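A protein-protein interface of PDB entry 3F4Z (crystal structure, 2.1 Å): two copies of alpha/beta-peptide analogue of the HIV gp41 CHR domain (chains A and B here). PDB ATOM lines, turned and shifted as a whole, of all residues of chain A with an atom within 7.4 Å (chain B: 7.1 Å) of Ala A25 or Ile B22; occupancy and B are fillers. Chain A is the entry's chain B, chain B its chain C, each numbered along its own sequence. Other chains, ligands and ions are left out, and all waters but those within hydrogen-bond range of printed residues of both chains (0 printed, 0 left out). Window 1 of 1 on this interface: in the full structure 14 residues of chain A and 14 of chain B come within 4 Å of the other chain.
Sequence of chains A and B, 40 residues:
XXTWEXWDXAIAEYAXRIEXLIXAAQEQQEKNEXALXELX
ND2 of Asn A32 lies within hydrogen-bond range of O of Ala B25. The side-chain amide oxygen (OE1) of Gln A28 lies close to the side-chain amide nitrogen (NE2) of Gln B26 (3.3 Å).
The side-chain amide nitrogen (NE2) of Gln A28 lies within hydrogen-bond range of the side-chain amide oxygen (OD1) of Asn A32 (2.5 Å).
CD1 of Leu A21 touches CB of Ala B15, at 3.5 Å. Leu A21 touches Ile B18. CD2 of Leu A21 touches CG of Glu B19 (3.9 Å). Ala A24 touches Ile B22. Ile B22 touches Ala A25. CG of Gln A28 touches CB of Ala B25, 3.5 Å away. Asn A32 touches Gln B28 (ND2 to CB, 3.7 Å).
Ala A25 touches one residue of chain B. Printed residues of chain B within 4 Å of Asn A32: Ala B25 (3.1 Å) and Gln B28 (3.7 Å). Printed residues of chain B within 4 Å of Leu A21: Ala B15, Ile B18 and Glu B19. The nearest residue of chain B that does not touch Ala A25 is Ile B18 (5.1 Å). The nearest residue of chain A that does not touch Ile B22 is Leu A21 (4.02 Å). The nearest printed residue of chain A that does not touch Glu B19 is Ala A24 (7.3 Å).
Along chain B the printed residues that touch a printed residue of chain A span positions 15 to 28. Among the printed residues, no Asp or Glu carboxylate lies within 4 Å of a Lys or Arg side-chain nitrogen of the other chain.
Ala A24 touches Ile B22, but with the chains exchanged Ile A22 does not touch Ala B24 (12.0 Å). Ala A25 touches Ile B22, but with the chains exchanged Ile A22 does not touch Ala B25 (9.9 Å). Gln A28 touches Ala B25, but with the chains exchanged Ala A25 does not touch Gln B28 (9.1 Å). Gln A28 touches Gln B26, but with the chains exchanged Gln A26 does not touch Gln B28 (11.2 Å). 10 positions are printed for both chains.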
ATOM      1  N   GLU A  19     -36.220  -1.878  14.852  1.00  0.00           N
ATOM      2  CA  GLU A  19     -35.695  -3.160  14.393  1.00  0.00           C
ATOM      3  C   GLU A  19     -35.169  -3.113  12.965  1.00  0.00           C
ATOM      4  O   GLU A  19     -34.298  -3.884  12.601  1.00  0.00           O
ATOM      5  CB  GLU A  19     -36.660  -4.289  14.701  1.00  0.00           C
ATOM      6  CG  GLU A  19     -36.912  -4.311  16.210  1.00  0.00           C
ATOM      7  CD  GLU A  19     -37.827  -5.443  16.686  1.00  0.00           C
ATOM      8  OE1 GLU A  19     -37.698  -6.565  16.158  1.00  0.00           O
ATOM      9  OE2 GLU A  19     -38.625  -5.217  17.632  1.00  0.00           O
ATOM     10  N   XCP A  20     -35.704  -2.206  12.166  1.00  0.00           N
ATOM     11  CB  XCP A  20     -35.293  -2.049  10.772  1.00  0.00           C
ATOM     12  CG  XCP A  20     -36.412  -2.034   9.711  1.00  0.00           C
ATOM     13  CD  XCP A  20     -36.170  -0.768   8.871  1.00  0.00           C
ATOM     14  CE  XCP A  20     -34.791  -0.213   9.289  1.00  0.00           C
ATOM     15  CA  XCP A  20     -34.660  -0.621  10.763  1.00  0.00           C
ATOM     16  C   XCP A  20     -33.233  -0.525  11.333  1.00  0.00           C
ATOM     17  O   XCP A  20     -32.277  -0.973  10.737  1.00  0.00           O
ATOM     18  N   LEU A  21     -33.093   0.084  12.533  1.00  0.00           N
ATOM     19  CA  LEU A  21     -31.764   0.235  13.183  1.00  0.00           C
ATOM     20  C   LEU A  21     -31.062  -1.057  13.594  1.00  0.00           C
ATOM     21  O   LEU A  21     -29.850  -1.185  13.431  1.00  0.00           O
ATOM     22  CB  LEU A  21     -31.856   1.168  14.403  1.00  0.00           C
ATOM     23  CG  LEU A  21     -31.846   2.649  13.995  1.00  0.00           C
ATOM     24  CD1 LEU A  21     -32.242   3.469  15.202  1.00  0.00           C
ATOM     25  CD2 LEU A  21     -30.467   3.102  13.380  1.00  0.00           C
ATOM     26  N   ILE A  22     -31.781  -2.013  14.173  1.00  0.00           N
ATOM     27  CA  ILE A  22     -31.089  -3.225  14.600  1.00  0.00           C
ATOM     28  C   ILE A  22     -30.579  -3.989  13.371  1.00  0.00           C
ATOM     29  O   ILE A  22     -29.435  -4.449  13.333  1.00  0.00           O
ATOM     30  CB  ILE A  22     -31.956  -4.111  15.521  1.00  0.00           C
ATOM     31  CG1 ILE A  22     -32.242  -3.403  16.880  1.00  0.00           C
ATOM     32  CG2 ILE A  22     -31.274  -5.458  15.772  1.00  0.00           C
ATOM     33  CD1 ILE A  22     -30.991  -3.277  17.821  1.00  0.00           C
ATOM     34  N   XPC A  23     -31.436  -4.126  12.355  1.00  0.00           N
ATOM     35  CB  XPC A  23     -31.025  -4.839  11.153  1.00  0.00           C
ATOM     36  CG  XPC A  23     -32.197  -5.610  10.519  1.00  0.00           C
ATOM     37  ND  XPC A  23     -31.912  -5.593   9.015  1.00  0.00           N
ATOM     38  CE  XPC A  23     -30.688  -4.736   8.753  1.00  0.00           C
ATOM     39  CA  XPC A  23     -30.635  -3.851  10.022  1.00  0.00           C
ATOM     40  C   XPC A  23     -29.268  -3.196  10.085  1.00  0.00           C
ATOM     41  O   XPC A  23     -28.275  -3.839   9.850  1.00  0.00           O
ATOM     42  N   ALA A  24     -29.227  -1.914  10.403  1.00  0.00           N
ATOM     43  CA  ALA A  24     -27.957  -1.199  10.486  1.00  0.00           C
ATOM     44  C   ALA A  24     -26.935  -1.802  11.450  1.00  0.00           C
ATOM     45  O   ALA A  24     -25.763  -1.907  11.107  1.00  0.00           O
ATOM     46  CB  ALA A  24     -28.219   0.280  10.799  1.00  0.00           C
ATOM     47  N   ALA A  25     -27.350  -2.255  12.633  1.00  0.00           N
ATOM     48  CA  ALA A  25     -26.329  -2.787  13.588  1.00  0.00           C
ATOM     49  C   ALA A  25     -25.741  -4.116  13.149  1.00  0.00           C
ATOM     50  O   ALA A  25     -24.537  -4.363  13.348  1.00  0.00           O
ATOM     51  CB  ALA A  25     -26.881  -2.912  15.028  1.00  0.00           C
ATOM     52  N   GLN A  26     -26.586  -4.984  12.606  1.00  0.00           N
ATOM     53  CA  GLN A  26     -26.158  -6.333  12.205  1.00  0.00           C
ATOM     54  C   GLN A  26     -25.347  -6.311  10.892  1.00  0.00           C
ATOM     55  O   GLN A  26     -24.408  -7.102  10.729  1.00  0.00           O
ATOM     56  CB  GLN A  26     -27.384  -7.258  12.022  1.00  0.00           C
ATOM     57  N   B3E A  27     -25.724  -5.415   9.995  1.00  0.00           N
ATOM     58  CA  B3E A  27     -25.077  -5.250   8.700  1.00  0.00           C
ATOM     59  CG  B3E A  27     -26.150  -5.292   7.601  1.00  0.00           C
ATOM     60  CD  B3E A  27     -26.973  -6.546   7.705  1.00  0.00           C
ATOM     61  CE  B3E A  27     -28.052  -6.667   6.613  1.00  0.00           C
ATOM     62  OF2 B3E A  27     -28.280  -5.742   5.847  1.00  0.00           O
ATOM     63  OF1 B3E A  27     -28.698  -7.718   6.513  1.00  0.00           O
ATOM     64  CB  B3E A  27     -24.473  -3.909   8.517  1.00  0.00           C
ATOM     65  C   B3E A  27     -23.144  -3.804   9.236  1.00  0.00           C
ATOM     66  O   B3E A  27     -22.142  -4.292   8.764  1.00  0.00           O
ATOM     67  N   GLN A  28     -23.141  -3.153  10.399  1.00  0.00           N
ATOM     68  CA  GLN A  28     -21.919  -2.994  11.167  1.00  0.00           C
ATOM     69  C   GLN A  28     -21.301  -4.269  11.682  1.00  0.00           C
ATOM     70  O   GLN A  28     -20.103  -4.393  11.613  1.00  0.00           O
ATOM     71  CB  GLN A  28     -22.153  -2.030  12.328  1.00  0.00           C
ATOM     72  CG  GLN A  28     -20.884  -1.670  13.119  1.00  0.00           C
ATOM     73  CD  GLN A  28     -19.798  -1.141  12.226  1.00  0.00           C
ATOM     74  OE1 GLN A  28     -20.054  -0.296  11.384  1.00  0.00           O
ATOM     75  NE2 GLN A  28     -18.587  -1.660  12.374  1.00  0.00           N
ATOM     76  N   GLN A  29     -22.089  -5.211  12.204  1.00  0.00           N
ATOM     77  CA  GLN A  29     -21.503  -6.445  12.735  1.00  0.00           C
ATOM     78  C   GLN A  29     -20.870  -7.312  11.616  1.00  0.00           C
ATOM     79  O   GLN A  29     -19.747  -7.825  11.769  1.00  0.00           O
ATOM     80  CB  GLN A  29     -22.541  -7.261  13.517  1.00  0.00           C
ATOM     81  CG  GLN A  29     -22.021  -8.620  13.986  1.00  0.00           C
ATOM     82  CD  GLN A  29     -20.826  -8.536  14.975  1.00  0.00           C
ATOM     83  OE1 GLN A  29     -20.671  -7.578  15.730  1.00  0.00           O
ATOM     84  NE2 GLN A  29     -19.993  -9.553  14.955  1.00  0.00           N
ATOM     85  N   B3E A  30     -21.600  -7.466  10.500  1.00  0.00           N
ATOM     86  CA  B3E A  30     -21.130  -8.254   9.368  1.00  0.00           C
ATOM     87  CG  B3E A  30     -22.285  -9.065   8.804  1.00  0.00           C
ATOM     88  CD  B3E A  30     -22.862 -10.065   9.782  1.00  0.00           C
ATOM     89  CE  B3E A  30     -24.250 -10.503   9.305  1.00  0.00           C
ATOM     90  OF2 B3E A  30     -25.124 -10.747  10.178  1.00  0.00           O
ATOM     91  OF1 B3E A  30     -24.476 -10.602   8.062  1.00  0.00           O
ATOM     92  CB  B3E A  30     -20.702  -7.374   8.224  1.00  0.00           C
ATOM     93  C   B3E A  30     -19.347  -6.739   8.396  1.00  0.00           C
ATOM     94  O   B3E A  30     -18.351  -7.416   8.305  1.00  0.00           O
ATOM     95  N   LYS A  31     -19.310  -5.446   8.643  1.00  0.00           N
ATOM     96  CA  LYS A  31     -18.046  -4.755   8.821  1.00  0.00           C
ATOM     97  C   LYS A  31     -17.093  -5.303   9.867  1.00  0.00           C
ATOM     98  O   LYS A  31     -15.926  -5.417   9.566  1.00  0.00           O
ATOM     99  CB  LYS A  31     -18.244  -3.264   9.039  1.00  0.00           C
ATOM    100  CG  LYS A  31     -18.752  -2.515   7.807  1.00  0.00           C
ATOM    101  CD  LYS A  31     -18.951  -1.045   8.122  1.00  0.00           C
ATOM    102  CE  LYS A  31     -19.483  -0.254   6.925  1.00  0.00           C
ATOM    103  NZ  LYS A  31     -20.108   1.067   7.335  1.00  0.00           N
ATOM    104  N   ASN A  32     -17.561  -5.641  11.069  1.00  0.00           N
ATOM    105  CA  ASN A  32     -16.651  -6.123  12.119  1.00  0.00           C
ATOM    106  C   ASN A  32     -16.115  -7.518  11.808  1.00  0.00           C
ATOM    107  O   ASN A  32     -14.967  -7.827  12.115  1.00  0.00           O
ATOM    108  CB  ASN A  32     -17.297  -6.102  13.514  1.00  0.00           C
ATOM    109  CG  ASN A  32     -17.422  -4.689  14.095  1.00  0.00           C
ATOM    110  OD1 ASN A  32     -17.469  -3.705  13.367  1.00  0.00           O
ATOM    111  ND2 ASN A  32     -17.456  -4.591  15.398  1.00  0.00           N
ATOM    112  N   ALA B  15     -33.666   4.939  19.904  1.00  0.00           N
ATOM    113  CA  ALA B  15     -33.042   4.860  18.587  1.00  0.00           C
ATOM    114  C   ALA B  15     -31.643   5.533  18.613  1.00  0.00           C
ATOM    115  O   ALA B  15     -30.649   4.981  18.149  1.00  0.00           O
ATOM    116  CB  ALA B  15     -33.949   5.535  17.523  1.00  0.00           C
ATOM    117  N   XCP B  16     -31.599   6.727  19.162  1.00  0.00           N
ATOM    118  CB  XCP B  16     -30.348   7.510  19.268  1.00  0.00           C
ATOM    119  CG  XCP B  16     -30.579   8.996  18.918  1.00  0.00           C
ATOM    120  CD  XCP B  16     -29.500   9.811  19.689  1.00  0.00           C
ATOM    121  CE  XCP B  16     -28.955   8.846  20.769  1.00  0.00           C
ATOM    122  CA  XCP B  16     -29.815   7.553  20.684  1.00  0.00           C
ATOM    123  C   XCP B  16     -29.030   6.302  21.077  1.00  0.00           C
ATOM    124  O   XCP B  16     -27.908   6.111  20.646  1.00  0.00           O
ATOM    125  N   ARG B  17     -29.656   5.447  21.916  1.00  0.00           N
ATOM    126  CA  ARG B  17     -29.051   4.215  22.388  1.00  0.00           C
ATOM    127  C   ARG B  17     -28.539   3.238  21.360  1.00  0.00           C
ATOM    128  O   ARG B  17     -27.452   2.673  21.527  1.00  0.00           O
ATOM    129  CB  ARG B  17     -29.984   3.537  23.421  1.00  0.00           C
ATOM    130  CG  ARG B  17     -30.023   4.420  24.704  1.00  0.00           C
ATOM    131  CD  ARG B  17     -30.905   3.910  25.841  1.00  0.00           C
ATOM    132  NE  ARG B  17     -30.468   2.597  26.247  1.00  0.00           N
ATOM    133  CZ  ARG B  17     -31.180   1.772  27.019  1.00  0.00           C
ATOM    134  NH1 ARG B  17     -32.360   2.154  27.503  1.00  0.00           N
ATOM    135  NH2 ARG B  17     -30.702   0.556  27.297  1.00  0.00           N
ATOM    136  N   ILE B  18     -29.277   3.064  20.279  1.00  0.00           N
ATOM    137  CA  ILE B  18     -28.868   2.122  19.257  1.00  0.00           C
ATOM    138  C   ILE B  18     -27.832   2.746  18.309  1.00  0.00           C
ATOM    139  O   ILE B  18     -26.800   2.129  18.069  1.00  0.00           O
ATOM    140  CB  ILE B  18     -30.088   1.527  18.511  1.00  0.00           C
ATOM    141  CG1 ILE B  18     -30.919   0.682  19.490  1.00  0.00           C
ATOM    142  CG2 ILE B  18     -29.663   0.655  17.314  1.00  0.00           C
ATOM    143  CD1 ILE B  18     -32.255   0.391  18.997  1.00  0.00           C
ATOM    144  N   GLU B  19     -28.079   3.947  17.785  1.00  0.00           N
ATOM    145  CA  GLU B  19     -27.022   4.637  17.007  1.00  0.00           C
ATOM    146  C   GLU B  19     -25.724   4.831  17.792  1.00  0.00           C
ATOM    147  O   GLU B  19     -24.638   4.706  17.227  1.00  0.00           O
ATOM    148  CB  GLU B  19     -27.525   5.966  16.494  1.00  0.00           C
ATOM    149  CG  GLU B  19     -28.672   5.784  15.547  1.00  0.00           C
ATOM    150  CD  GLU B  19     -29.411   7.054  15.272  1.00  0.00           C
ATOM    151  OE1 GLU B  19     -29.080   8.096  15.878  1.00  0.00           O
ATOM    152  OE2 GLU B  19     -30.308   7.006  14.408  1.00  0.00           O
ATOM    153  N   XCP B  20     -25.837   5.131  19.072  1.00  0.00           N
ATOM    154  CB  XCP B  20     -24.685   5.344  19.942  1.00  0.00           C
ATOM    155  CG  XCP B  20     -24.764   6.714  20.603  1.00  0.00           C
ATOM    156  CD  XCP B  20     -24.299   6.492  22.051  1.00  0.00           C
ATOM    157  CE  XCP B  20     -23.891   5.021  22.224  1.00  0.00           C
ATOM    158  CA  XCP B  20     -24.667   4.316  21.110  1.00  0.00           C
ATOM    159  C   XCP B  20     -24.016   2.998  20.700  1.00  0.00           C
ATOM    160  O   XCP B  20     -22.793   2.945  20.544  1.00  0.00           O
ATOM    161  N   LEU B  21     -24.820   1.942  20.525  1.00  0.00           N
ATOM    162  CA  LEU B  21     -24.311   0.611  20.128  1.00  0.00           C
ATOM    163  C   LEU B  21     -23.482   0.600  18.849  1.00  0.00           C
ATOM    164  O   LEU B  21     -22.410  -0.003  18.804  1.00  0.00           O
ATOM    165  CB  LEU B  21     -25.446  -0.382  19.894  1.00  0.00           C
ATOM    166  CG  LEU B  21     -26.233  -0.768  21.125  1.00  0.00           C
ATOM    167  CD1 LEU B  21     -27.460  -1.625  20.746  1.00  0.00           C
ATOM    168  CD2 LEU B  21     -25.293  -1.453  22.169  1.00  0.00           C
ATOM    169  N   ILE B  22     -24.007   1.231  17.802  1.00  0.00           N
ATOM    170  CA  ILE B  22     -23.380   1.130  16.494  1.00  0.00           C
ATOM    171  C   ILE B  22     -22.083   1.972  16.491  1.00  0.00           C
ATOM    172  O   ILE B  22     -21.035   1.486  16.091  1.00  0.00           O
ATOM    173  CB  ILE B  22     -24.292   1.566  15.320  1.00  0.00           C
ATOM    174  CG1 ILE B  22     -25.507   0.625  15.221  1.00  0.00           C
ATOM    175  CG2 ILE B  22     -23.505   1.516  14.010  1.00  0.00           C
ATOM    176  CD1 ILE B  22     -26.620   1.078  14.227  1.00  0.00           C
ATOM    177  N   XPC B  23     -22.174   3.213  16.933  1.00  0.00           N
ATOM    178  CB  XPC B  23     -20.995   4.043  16.952  1.00  0.00           C
ATOM    179  CG  XPC B  23     -21.351   5.466  16.541  1.00  0.00           C
ATOM    180  ND  XPC B  23     -20.407   6.337  17.361  1.00  0.00           N
ATOM    181  CE  XPC B  23     -19.574   5.439  18.263  1.00  0.00           C
ATOM    182  CA  XPC B  23     -20.405   4.150  18.364  1.00  0.00           C
ATOM    183  C   XPC B  23     -19.556   2.993  18.788  1.00  0.00           C
ATOM    184  O   XPC B  23     -18.481   2.792  18.227  1.00  0.00           O
ATOM    185  N   ALA B  24     -20.038   2.235  19.775  1.00  0.00           N
ATOM    186  CA  ALA B  24     -19.324   1.081  20.290  1.00  0.00           C
ATOM    187  C   ALA B  24     -18.792   0.076  19.283  1.00  0.00           C
ATOM    188  O   ALA B  24     -17.624  -0.346  19.411  1.00  0.00           O
ATOM    189  CB  ALA B  24     -20.120   0.379  21.395  1.00  0.00           C
ATOM    190  N   ALA B  25     -19.608  -0.286  18.285  1.00  0.00           N
ATOM    191  CA  ALA B  25     -19.190  -1.296  17.320  1.00  0.00           C
ATOM    192  C   ALA B  25     -18.144  -0.759  16.347  1.00  0.00           C
ATOM    193  O   ALA B  25     -17.244  -1.506  15.961  1.00  0.00           O
ATOM    194  CB  ALA B  25     -20.395  -1.886  16.551  1.00  0.00           C
ATOM    195  N   GLN B  26     -18.318   0.477  15.868  1.00  0.00           N
ATOM    196  CA  GLN B  26     -17.374   1.087  14.967  1.00  0.00           C
ATOM    197  C   GLN B  26     -16.057   1.460  15.646  1.00  0.00           C
ATOM    198  O   GLN B  26     -15.020   1.340  15.044  1.00  0.00           O
ATOM    199  CB  GLN B  26     -17.964   2.334  14.306  1.00  0.00           C
ATOM    200  CG  GLN B  26     -19.028   2.019  13.270  1.00  0.00           C
ATOM    201  CD  GLN B  26     -19.901   3.194  12.849  1.00  0.00           C
ATOM    202  OE1 GLN B  26     -19.814   4.306  13.379  1.00  0.00           O
ATOM    203  NE2 GLN B  26     -20.785   2.927  11.893  1.00  0.00           N
ATOM    204  N   B3E B  27     -16.122   1.908  16.896  1.00  0.00           N
ATOM    205  CA  B3E B  27     -14.948   2.302  17.670  1.00  0.00           C
ATOM    206  CG  B3E B  27     -15.182   3.701  18.212  1.00  0.00           C
ATOM    207  CD  B3E B  27     -15.347   4.713  17.097  1.00  0.00           C
ATOM    208  CE  B3E B  27     -15.743   6.039  17.726  1.00  0.00           C
ATOM    209  OF2 B3E B  27     -15.818   7.069  17.021  1.00  0.00           O
ATOM    210  OF1 B3E B  27     -15.981   6.070  18.953  1.00  0.00           O
ATOM    211  CB  B3E B  27     -14.759   1.405  18.878  1.00  0.00           C
ATOM    212  C   B3E B  27     -14.077   0.124  18.488  1.00  0.00           C
ATOM    213  O   B3E B  27     -12.864   0.102  18.258  1.00  0.00           O
ATOM    214  N   GLN B  28     -14.865  -0.953  18.413  1.00  0.00           N
ATOM    215  CA  GLN B  28     -14.340  -2.271  18.045  1.00  0.00           C
ATOM    216  C   GLN B  28     -13.708  -2.370  16.680  1.00  0.00           C
ATOM    217  O   GLN B  28     -12.587  -2.858  16.586  1.00  0.00           O
ATOM    218  CB  GLN B  28     -15.374  -3.403  18.259  1.00  0.00           C
ATOM    219  CG  GLN B  28     -15.945  -3.359  19.699  1.00  0.00           C
ATOM    220  CD  GLN B  28     -16.777  -4.582  20.113  1.00  0.00           C
ATOM    221  OE1 GLN B  28     -17.785  -4.945  19.470  1.00  0.00           O
ATOM    222  NE2 GLN B  28     -16.380  -5.196  21.225  1.00  0.00           N
